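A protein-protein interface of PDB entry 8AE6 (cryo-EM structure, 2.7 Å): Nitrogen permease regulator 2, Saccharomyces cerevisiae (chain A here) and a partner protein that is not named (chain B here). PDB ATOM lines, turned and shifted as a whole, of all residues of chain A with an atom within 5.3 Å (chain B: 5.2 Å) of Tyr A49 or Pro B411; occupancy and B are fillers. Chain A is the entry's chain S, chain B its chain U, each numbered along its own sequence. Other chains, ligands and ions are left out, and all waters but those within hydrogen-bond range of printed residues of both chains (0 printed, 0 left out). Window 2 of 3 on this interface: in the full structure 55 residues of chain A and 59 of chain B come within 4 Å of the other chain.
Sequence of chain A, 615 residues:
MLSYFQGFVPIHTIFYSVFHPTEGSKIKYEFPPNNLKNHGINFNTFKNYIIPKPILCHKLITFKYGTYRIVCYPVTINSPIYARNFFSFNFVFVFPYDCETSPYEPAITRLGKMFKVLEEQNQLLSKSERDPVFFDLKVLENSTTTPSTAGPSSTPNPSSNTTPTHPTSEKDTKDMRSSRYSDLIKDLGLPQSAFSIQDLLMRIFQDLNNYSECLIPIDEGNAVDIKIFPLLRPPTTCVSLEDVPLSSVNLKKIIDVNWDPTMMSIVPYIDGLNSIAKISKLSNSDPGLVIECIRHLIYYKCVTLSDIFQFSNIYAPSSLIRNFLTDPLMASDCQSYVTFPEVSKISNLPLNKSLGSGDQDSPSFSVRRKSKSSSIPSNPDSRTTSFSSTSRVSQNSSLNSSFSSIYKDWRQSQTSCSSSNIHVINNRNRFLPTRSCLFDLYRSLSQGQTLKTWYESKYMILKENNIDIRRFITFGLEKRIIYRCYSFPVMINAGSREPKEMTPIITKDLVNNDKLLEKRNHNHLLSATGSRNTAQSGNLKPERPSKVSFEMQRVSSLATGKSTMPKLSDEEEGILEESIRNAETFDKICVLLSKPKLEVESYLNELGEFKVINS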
ATOM      1  N   PHE A  46     -12.469  16.766   6.190  1.00  0.00           N
ATOM      2  CA  PHE A  46     -11.692  15.578   5.858  1.00  0.00           C
ATOM      3  C   PHE A  46     -11.364  15.500   4.370  1.00  0.00           C
ATOM      4  O   PHE A  46     -11.165  14.410   3.832  1.00  0.00           O
ATOM      5  CB  PHE A  46     -12.409  14.306   6.314  1.00  0.00           C
ATOM      6  CG  PHE A  46     -13.832  14.179   5.830  1.00  0.00           C
ATOM      7  CD1 PHE A  46     -14.119  13.608   4.600  1.00  0.00           C
ATOM      8  CD2 PHE A  46     -14.885  14.590   6.626  1.00  0.00           C
ATOM      9  CE1 PHE A  46     -15.420  13.478   4.162  1.00  0.00           C
ATOM     10  CE2 PHE A  46     -16.189  14.458   6.196  1.00  0.00           C
ATOM     11  CZ  PHE A  46     -16.457  13.905   4.961  1.00  0.00           C
ATOM     12  N   LYS A  47     -11.293  16.650   3.693  1.00  0.00           N
ATOM     13  CA  LYS A  47     -10.971  16.653   2.271  1.00  0.00           C
ATOM     14  C   LYS A  47      -9.534  16.238   1.993  1.00  0.00           C
ATOM     15  O   LYS A  47      -9.230  15.821   0.872  1.00  0.00           O
ATOM     16  CB  LYS A  47     -11.234  18.034   1.672  1.00  0.00           C
ATOM     17  CG  LYS A  47     -10.451  19.157   2.326  1.00  0.00           C
ATOM     18  CD  LYS A  47     -10.666  20.473   1.599  1.00  0.00           C
ATOM     19  CE  LYS A  47      -9.772  20.579   0.376  1.00  0.00           C
ATOM     20  NZ  LYS A  47      -9.884  21.908  -0.281  1.00  0.00           N
ATOM     21  N   ASN A  48      -8.647  16.338   2.982  1.00  0.00           N
ATOM     22  CA  ASN A  48      -7.256  15.947   2.814  1.00  0.00           C
ATOM     23  C   ASN A  48      -7.025  14.456   3.019  1.00  0.00           C
ATOM     24  O   ASN A  48      -5.909  13.984   2.794  1.00  0.00           O
ATOM     25  CB  ASN A  48      -6.365  16.740   3.769  1.00  0.00           C
ATOM     26  CG  ASN A  48      -6.079  18.139   3.269  1.00  0.00           C
ATOM     27  OD1 ASN A  48      -5.830  18.345   2.083  1.00  0.00           O
ATOM     28  ND2 ASN A  48      -6.117  19.112   4.174  1.00  0.00           N
ATOM     29  N   TYR A  49      -8.041  13.715   3.457  1.00  0.00           N
ATOM     30  CA  TYR A  49      -7.983  12.258   3.474  1.00  0.00           C
ATOM     31  C   TYR A  49      -8.653  11.634   2.263  1.00  0.00           C
ATOM     32  O   TYR A  49      -8.247  10.548   1.834  1.00  0.00           O
ATOM     33  CB  TYR A  49      -8.643  11.707   4.742  1.00  0.00           C
ATOM     34  CG  TYR A  49      -8.028  12.200   6.030  1.00  0.00           C
ATOM     35  CD1 TYR A  49      -6.656  12.355   6.155  1.00  0.00           C
ATOM     36  CD2 TYR A  49      -8.825  12.501   7.126  1.00  0.00           C
ATOM     37  CE1 TYR A  49      -6.094  12.805   7.334  1.00  0.00           C
ATOM     38  CE2 TYR A  49      -8.274  12.947   8.308  1.00  0.00           C
ATOM     39  CZ  TYR A  49      -6.908  13.100   8.406  1.00  0.00           C
ATOM     40  OH  TYR A  49      -6.354  13.545   9.584  1.00  0.00           O
ATOM     41  N   ILE A  50      -9.676  12.295   1.716  1.00  0.00           N
ATOM     42  CA  ILE A  50     -10.337  11.802   0.512  1.00  0.00           C
ATOM     43  C   ILE A  50      -9.403  11.913  -0.688  1.00  0.00           C
ATOM     44  O   ILE A  50      -9.263  10.970  -1.476  1.00  0.00           O
ATOM     45  CB  ILE A  50     -11.654  12.564   0.281  1.00  0.00           C
ATOM     46  CG1 ILE A  50     -12.555  12.444   1.507  1.00  0.00           C
ATOM     47  CG2 ILE A  50     -12.366  12.040  -0.948  1.00  0.00           C
ATOM     48  CD1 ILE A  50     -12.967  11.034   1.830  1.00  0.00           C
ATOM     49  N   ILE A  51      -8.749  13.059  -0.841  1.00  0.00           N
ATOM     50  CA  ILE A  51      -7.713  13.235  -1.855  1.00  0.00           C
ATOM     51  C   ILE A  51      -6.402  13.523  -1.134  1.00  0.00           C
ATOM     52  O   ILE A  51      -6.009  14.691  -0.999  1.00  0.00           O
ATOM     53  CB  ILE A  51      -8.067  14.353  -2.849  1.00  0.00           C
ATOM     54  CG1 ILE A  51      -9.521  14.236  -3.308  1.00  0.00           C
ATOM     55  CG2 ILE A  51      -7.138  14.316  -4.050  1.00  0.00           C
ATOM     56  CD1 ILE A  51      -9.793  13.030  -4.178  1.00  0.00           C
ATOM     57  N   PRO A  52      -5.710  12.501  -0.635  1.00  0.00           N
ATOM     58  CA  PRO A  52      -4.466  12.738   0.098  1.00  0.00           C
ATOM     59  C   PRO A  52      -3.256  12.819  -0.813  1.00  0.00           C
ATOM     60  O   PRO A  52      -3.385  12.840  -2.041  1.00  0.00           O
ATOM     61  CB  PRO A  52      -4.384  11.527   1.031  1.00  0.00           C
ATOM     62  CG  PRO A  52      -5.100  10.433   0.282  1.00  0.00           C
ATOM     63  CD  PRO A  52      -6.001  11.064  -0.755  1.00  0.00           C
ATOM     64  N   LEU A  56      -0.462   8.079   0.601  1.00  0.00           N
ATOM     65  CA  LEU A  56      -1.691   7.505   1.133  1.00  0.00           C
ATOM     66  C   LEU A  56      -2.638   7.006   0.051  1.00  0.00           C
ATOM     67  O   LEU A  56      -3.595   6.294   0.373  1.00  0.00           O
ATOM     68  CB  LEU A  56      -2.426   8.528   1.997  1.00  0.00           C
ATOM     69  CG  LEU A  56      -2.080   8.603   3.480  1.00  0.00           C
ATOM     70  CD1 LEU A  56      -3.088   9.468   4.215  1.00  0.00           C
ATOM     71  CD2 LEU A  56      -2.015   7.221   4.086  1.00  0.00           C
ATOM     72  N   ILE A  61      -8.602   3.587   2.852  1.00  0.00           N
ATOM     73  CA  ILE A  61      -8.608   4.568   3.929  1.00  0.00           C
ATOM     74  C   ILE A  61      -9.996   4.584   4.546  1.00  0.00           C
ATOM     75  O   ILE A  61     -10.994   4.810   3.853  1.00  0.00           O
ATOM     76  CB  ILE A  61      -8.210   5.964   3.423  1.00  0.00           C
ATOM     77  CG1 ILE A  61      -6.756   5.972   2.959  1.00  0.00           C
ATOM     78  CG2 ILE A  61      -8.427   7.004   4.504  1.00  0.00           C
ATOM     79  CD1 ILE A  61      -5.763   5.694   4.058  1.00  0.00           C
ATOM     80  N   PHE A  63     -11.931   6.195   8.083  1.00  0.00           N
ATOM     81  CA  PHE A  63     -11.804   7.047   9.255  1.00  0.00           C
ATOM     82  C   PHE A  63     -13.182   7.336   9.826  1.00  0.00           C
ATOM     83  O   PHE A  63     -14.203   7.196   9.151  1.00  0.00           O
ATOM     84  CB  PHE A  63     -11.059   8.357   8.943  1.00  0.00           C
ATOM     85  CG  PHE A  63     -11.622   9.131   7.781  1.00  0.00           C
ATOM     86  CD1 PHE A  63     -11.175   8.894   6.490  1.00  0.00           C
ATOM     87  CD2 PHE A  63     -12.573  10.118   7.986  1.00  0.00           C
ATOM     88  CE1 PHE A  63     -11.681   9.608   5.428  1.00  0.00           C
ATOM     89  CE2 PHE A  63     -13.081  10.831   6.926  1.00  0.00           C
ATOM     90  CZ  PHE A  63     -12.636  10.578   5.645  1.00  0.00           C
ATOM     91  N   CYS A  72     -13.139   4.744   2.026  1.00  0.00           N
ATOM     92  CA  CYS A  72     -12.792   5.245   0.708  1.00  0.00           C
ATOM     93  C   CYS A  72     -11.538   4.547   0.209  1.00  0.00           C
ATOM     94  O   CYS A  72     -10.734   4.028   0.988  1.00  0.00           O
ATOM     95  CB  CYS A  72     -12.581   6.761   0.719  1.00  0.00           C
ATOM     96  SG  CYS A  72     -11.289   7.350   1.823  1.00  0.00           S
ATOM     97  N   PRO A  74      -8.866   6.059  -2.233  1.00  0.00           N
ATOM     98  CA  PRO A  74      -8.375   7.144  -3.091  1.00  0.00           C
ATOM     99  C   PRO A  74      -7.466   6.633  -4.192  1.00  0.00           C
ATOM    100  O   PRO A  74      -6.612   5.772  -3.972  1.00  0.00           O
ATOM    101  CB  PRO A  74      -7.617   8.049  -2.117  1.00  0.00           C
ATOM    102  CG  PRO A  74      -7.280   7.176  -0.968  1.00  0.00           C
ATOM    103  CD  PRO A  74      -8.418   6.221  -0.841  1.00  0.00           C
ATOM    104  N   ASN A  90     -12.070   9.679  -5.962  1.00  0.00           N
ATOM    105  CA  ASN A  90     -12.338   8.776  -4.846  1.00  0.00           C
ATOM    106  C   ASN A  90     -13.818   8.431  -4.841  1.00  0.00           C
ATOM    107  O   ASN A  90     -14.660   9.326  -4.745  1.00  0.00           O
ATOM    108  CB  ASN A  90     -11.935   9.413  -3.520  1.00  0.00           C
ATOM    109  CG  ASN A  90     -11.632   8.389  -2.450  1.00  0.00           C
ATOM    110  OD1 ASN A  90     -12.039   7.232  -2.548  1.00  0.00           O
ATOM    111  ND2 ASN A  90     -10.911   8.809  -1.419  1.00  0.00           N
ATOM    112  N   GLU B 407       1.384  15.172   9.636  1.00  0.00           N
ATOM    113  CA  GLU B 407       0.354  15.815   8.834  1.00  0.00           C
ATOM    114  C   GLU B 407      -0.990  15.110   8.984  1.00  0.00           C
ATOM    115  O   GLU B 407      -2.007  15.754   9.263  1.00  0.00           O
ATOM    116  CB  GLU B 407       0.782  15.864   7.364  1.00  0.00           C
ATOM    117  CG  GLU B 407      -0.260  16.462   6.436  1.00  0.00           C
ATOM    118  CD  GLU B 407       0.333  16.934   5.122  1.00  0.00           C
ATOM    119  OE1 GLU B 407       1.411  16.431   4.741  1.00  0.00           O
ATOM    120  OE2 GLU B 407      -0.278  17.807   4.473  1.00  0.00           O
ATOM    121  N   PHE B 408      -1.027  13.785   8.813  1.00  0.00           N
ATOM    122  CA  PHE B 408      -2.333  13.129   8.832  1.00  0.00           C
ATOM    123  C   PHE B 408      -2.757  12.642  10.214  1.00  0.00           C
ATOM    124  O   PHE B 408      -3.858  12.103  10.343  1.00  0.00           O
ATOM    125  CB  PHE B 408      -2.411  11.983   7.787  1.00  0.00           C
ATOM    126  CG  PHE B 408      -1.677  10.704   8.150  1.00  0.00           C
ATOM    127  CD1 PHE B 408      -2.281   9.711   8.912  1.00  0.00           C
ATOM    128  CD2 PHE B 408      -0.423  10.451   7.632  1.00  0.00           C
ATOM    129  CE1 PHE B 408      -1.616   8.543   9.213  1.00  0.00           C
ATOM    130  CE2 PHE B 408       0.247   9.278   7.923  1.00  0.00           C
ATOM    131  CZ  PHE B 408      -0.353   8.325   8.714  1.00  0.00           C
ATOM    132  N   CYS B 409      -1.935  12.816  11.248  1.00  0.00           N
ATOM    133  CA  CYS B 409      -2.357  12.531  12.615  1.00  0.00           C
ATOM    134  C   CYS B 409      -2.606  13.800  13.421  1.00  0.00           C
ATOM    135  O   CYS B 409      -2.793  13.723  14.639  1.00  0.00           O
ATOM    136  CB  CYS B 409      -1.336  11.650  13.336  1.00  0.00           C
ATOM    137  SG  CYS B 409      -1.076  10.035  12.580  1.00  0.00           S
ATOM    138  N   SER B 410      -2.612  14.962  12.769  1.00  0.00           N
ATOM    139  CA  SER B 410      -2.947  16.239  13.395  1.00  0.00           C
ATOM    140  C   SER B 410      -4.153  16.795  12.650  1.00  0.00           C
ATOM    141  O   SER B 410      -4.005  17.613  11.727  1.00  0.00           O
ATOM    142  CB  SER B 410      -1.773  17.214  13.356  1.00  0.00           C
ATOM    143  OG  SER B 410      -1.578  17.721  12.047  1.00  0.00           O
ATOM    144  N   PRO B 411      -5.355  16.380  13.017  1.00  0.00           N
ATOM    145  CA  PRO B 411      -6.548  16.752  12.254  1.00  0.00           C
ATOM    146  C   PRO B 411      -7.026  18.154  12.617  1.00  0.00           C
ATOM    147  O   PRO B 411      -6.425  18.859  13.423  1.00  0.00           O
ATOM    148  CB  PRO B 411      -7.560  15.685  12.666  1.00  0.00           C
ATOM    149  CG  PRO B 411      -7.169  15.326  14.051  1.00  0.00           C
ATOM    150  CD  PRO B 411      -5.679  15.498  14.152  1.00  0.00           C
ATOM    151  N   GLU B 412      -8.137  18.546  11.998  1.00  0.00           N
ATOM    152  CA  GLU B 412      -8.722  19.858  12.210  1.00  0.00           C
ATOM    153  C   GLU B 412      -9.422  19.915  13.566  1.00  0.00           C
ATOM    154  O   GLU B 412      -9.515  18.921  14.291  1.00  0.00           O
ATOM    155  CB  GLU B 412      -9.690  20.194  11.076  1.00  0.00           C
ATOM    156  CG  GLU B 412      -9.044  20.906   9.901  1.00  0.00           C
ATOM    157  CD  GLU B 412      -8.348  19.953   8.951  1.00  0.00           C
ATOM    158  OE1 GLU B 412      -8.588  18.730   9.050  1.00  0.00           O
ATOM    159  OE2 GLU B 412      -7.560  20.424   8.103  1.00  0.00           O
ATOM    160  N   ARG B 413      -9.925  21.104  13.909  1.00  0.00           N
ATOM    161  CA  ARG B 413     -10.545  21.310  15.213  1.00  0.00           C
ATOM    162  C   ARG B 413     -11.851  20.538  15.359  1.00  0.00           C
ATOM    163  O   ARG B 413     -12.241  20.194  16.481  1.00  0.00           O
ATOM    164  CB  ARG B 413     -10.789  22.802  15.447  1.00  0.00           C
ATOM    165  CG  ARG B 413      -9.576  23.551  15.969  1.00  0.00           C
ATOM    166  CD  ARG B 413      -9.975  24.875  16.604  1.00  0.00           C
ATOM    167  NE  ARG B 413     -11.245  24.780  17.318  1.00  0.00           N
ATOM    168  CZ  ARG B 413     -11.370  24.365  18.569  1.00  0.00           C
ATOM    169  NH1 ARG B 413     -10.320  23.995  19.285  1.00  0.00           N
ATOM    170  NH2 ARG B 413     -12.581  24.321  19.120  1.00  0.00           N
ATOM    171  N   MET B 415     -12.294  17.525  14.129  1.00  0.00           N
ATOM    172  CA  MET B 415     -11.881  16.145  14.332  1.00  0.00           C
ATOM    173  C   MET B 415     -10.960  15.970  15.532  1.00  0.00           C
ATOM    174  O   MET B 415     -10.449  14.868  15.749  1.00  0.00           O
ATOM    175  CB  MET B 415     -11.197  15.609  13.070  1.00  0.00           C
ATOM    176  CG  MET B 415     -12.122  15.457  11.877  1.00  0.00           C
ATOM    177  SD  MET B 415     -11.407  14.460  10.558  1.00  0.00           S
ATOM    178  CE  MET B 415     -11.096  12.923  11.421  1.00  0.00           C
ATOM    179  N   CYS B 416     -10.733  17.025  16.307  1.00  0.00           N
ATOM    180  CA  CYS B 416      -9.953  16.948  17.532  1.00  0.00           C
ATOM    181  C   CYS B 416     -10.873  16.934  18.747  1.00  0.00           C
ATOM    182  O   CYS B 416     -12.077  17.193  18.649  1.00  0.00           O
ATOM    183  CB  CYS B 416      -8.969  18.115  17.624  1.00  0.00           C
ATOM    184  SG  CYS B 416      -7.486  17.942  16.614  1.00  0.00           S
ATOM    185  N   PHE B 420      -9.995   9.738  17.245  1.00  0.00           N
ATOM    186  CA  PHE B 420      -9.291   9.729  15.969  1.00  0.00           C
ATOM    187  C   PHE B 420      -9.036   8.277  15.584  1.00  0.00           C
ATOM    188  O   PHE B 420      -8.067   7.663  16.033  1.00  0.00           O
ATOM    189  CB  PHE B 420      -7.986  10.513  16.044  1.00  0.00           C
ATOM    190  CG  PHE B 420      -7.237  10.565  14.747  1.00  0.00           C
ATOM    191  CD1 PHE B 420      -7.626  11.432  13.745  1.00  0.00           C
ATOM    192  CD2 PHE B 420      -6.144   9.743  14.530  1.00  0.00           C
ATOM    193  CE1 PHE B 420      -6.943  11.481  12.551  1.00  0.00           C
ATOM    194  CE2 PHE B 420      -5.458   9.787  13.338  1.00  0.00           C
ATOM    195  CZ  PHE B 420      -5.858  10.654  12.349  1.00  0.00           C
ATOM    196  N   PHE B 422      -8.271   6.020  12.233  1.00  0.00           N
ATOM    197  CA  PHE B 422      -7.764   6.233  10.885  1.00  0.00           C
ATOM    198  C   PHE B 422      -6.975   5.003  10.476  1.00  0.00           C
ATOM    199  O   PHE B 422      -5.953   4.692  11.093  1.00  0.00           O
ATOM    200  CB  PHE B 422      -6.888   7.484  10.820  1.00  0.00           C
ATOM    201  CG  PHE B 422      -6.573   7.932   9.427  1.00  0.00           C
ATOM    202  CD1 PHE B 422      -7.491   8.666   8.700  1.00  0.00           C
ATOM    203  CD2 PHE B 422      -5.360   7.619   8.841  1.00  0.00           C
ATOM    204  CE1 PHE B 422      -7.208   9.077   7.414  1.00  0.00           C
ATOM    205  CE2 PHE B 422      -5.071   8.027   7.555  1.00  0.00           C
ATOM    206  CZ  PHE B 422      -5.995   8.757   6.842  1.00  0.00           C
ATOM    207  N   PRO B 433      -6.737  12.972  20.192  1.00  0.00           N
ATOM    208  CA  PRO B 433      -5.943  14.204  20.170  1.00  0.00           C
ATOM    209  C   PRO B 433      -6.600  15.286  21.000  1.00  0.00           C
ATOM    210  O   PRO B 433      -7.820  15.462  20.973  1.00  0.00           O
ATOM    211  CB  PRO B 433      -5.910  14.578  18.684  1.00  0.00           C
ATOM    212  CG  PRO B 433      -7.104  13.942  18.109  1.00  0.00           C
ATOM    213  CD  PRO B 433      -7.369  12.697  18.894  1.00  0.00           C
ATOM    214  N   MET B 532      -1.970  21.731  20.228  1.00  0.00           N
ATOM    215  CA  MET B 532      -2.451  20.371  20.031  1.00  0.00           C
ATOM    216  C   MET B 532      -1.333  19.398  20.365  1.00  0.00           C
ATOM    217  O   MET B 532      -0.174  19.642  20.028  1.00  0.00           O
ATOM    218  CB  MET B 532      -2.919  20.161  18.586  1.00  0.00           C
ATOM    219  CG  MET B 532      -3.940  19.049  18.387  1.00  0.00           C
ATOM    220  SD  MET B 532      -3.215  17.409  18.263  1.00  0.00           S
ATOM    221  CE  MET B 532      -2.002  17.682  16.983  1.00  0.00           C
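OH of Tyr A49 is in hydrogen-bond range of O of Phe B408 (3.0 Å).
The side-chain sulfur of Cys B416 sits at hydrogen-bond distance from the backbone carbonyl oxygen of Pro B411 (3.5 Å). The backbone carbonyl oxygen (O) of Ile A61 is in hydrogen-bond range of the backbone NH (N) of Cys A72 (2.8 Å).
Pro B411 touches Tyr A49 (CB to OH, 3.9 Å). Tyr A49 touches Phe B420. Tyr A49 touches Phe B422. Phe B422 touches Leu A56 (CZ to CD1, 3.98 Å). Ile A61 touches Phe B422. CD1 of Phe B422 touches CB of Phe A63, 3.6 Å away.
Tyr A49 touches just these residues of chain B: Phe B408 (3.0 Å), Pro B411 (3.9 Å), Phe B420 (3.7 Å) and Phe B422 (3.5 Å). Printed residues of chain B within 4 Å of Leu A56: Phe B422 (3.98 Å). Printed residues of chain B within 4 Å of Phe A63: Phe B422 (3.6 Å). Asn A90 touches none of the printed residues of chain B. Glu B407 touches none of the printed residues of chain A. Of the printed residues of chain A, Phe B408 touches Tyr A49 (3.0 Å). Of the printed residues of chain A, Phe B422 touches Tyr A49 (3.5 Å), Leu A56 (3.98 Å), Ile A61 (3.8 Å) and Phe A63 (3.6 Å). The nearest printed residue of chain A that does not touch Pro B411 is Phe A46 (8.0 Å).
Of the 13 printed residues of chain A, 4 touch a printed residue of chain B. Hydrophobic or aromatic side chains of chain B within 4 Å of the printed part of chain A: Phe B408, Pro B411, Phe B420 and Phe B422. Among the printed residues, no Asp or Glu carboxylate lies within 4 Å of a Lys or Arg side-chain nitrogen of the other chain.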
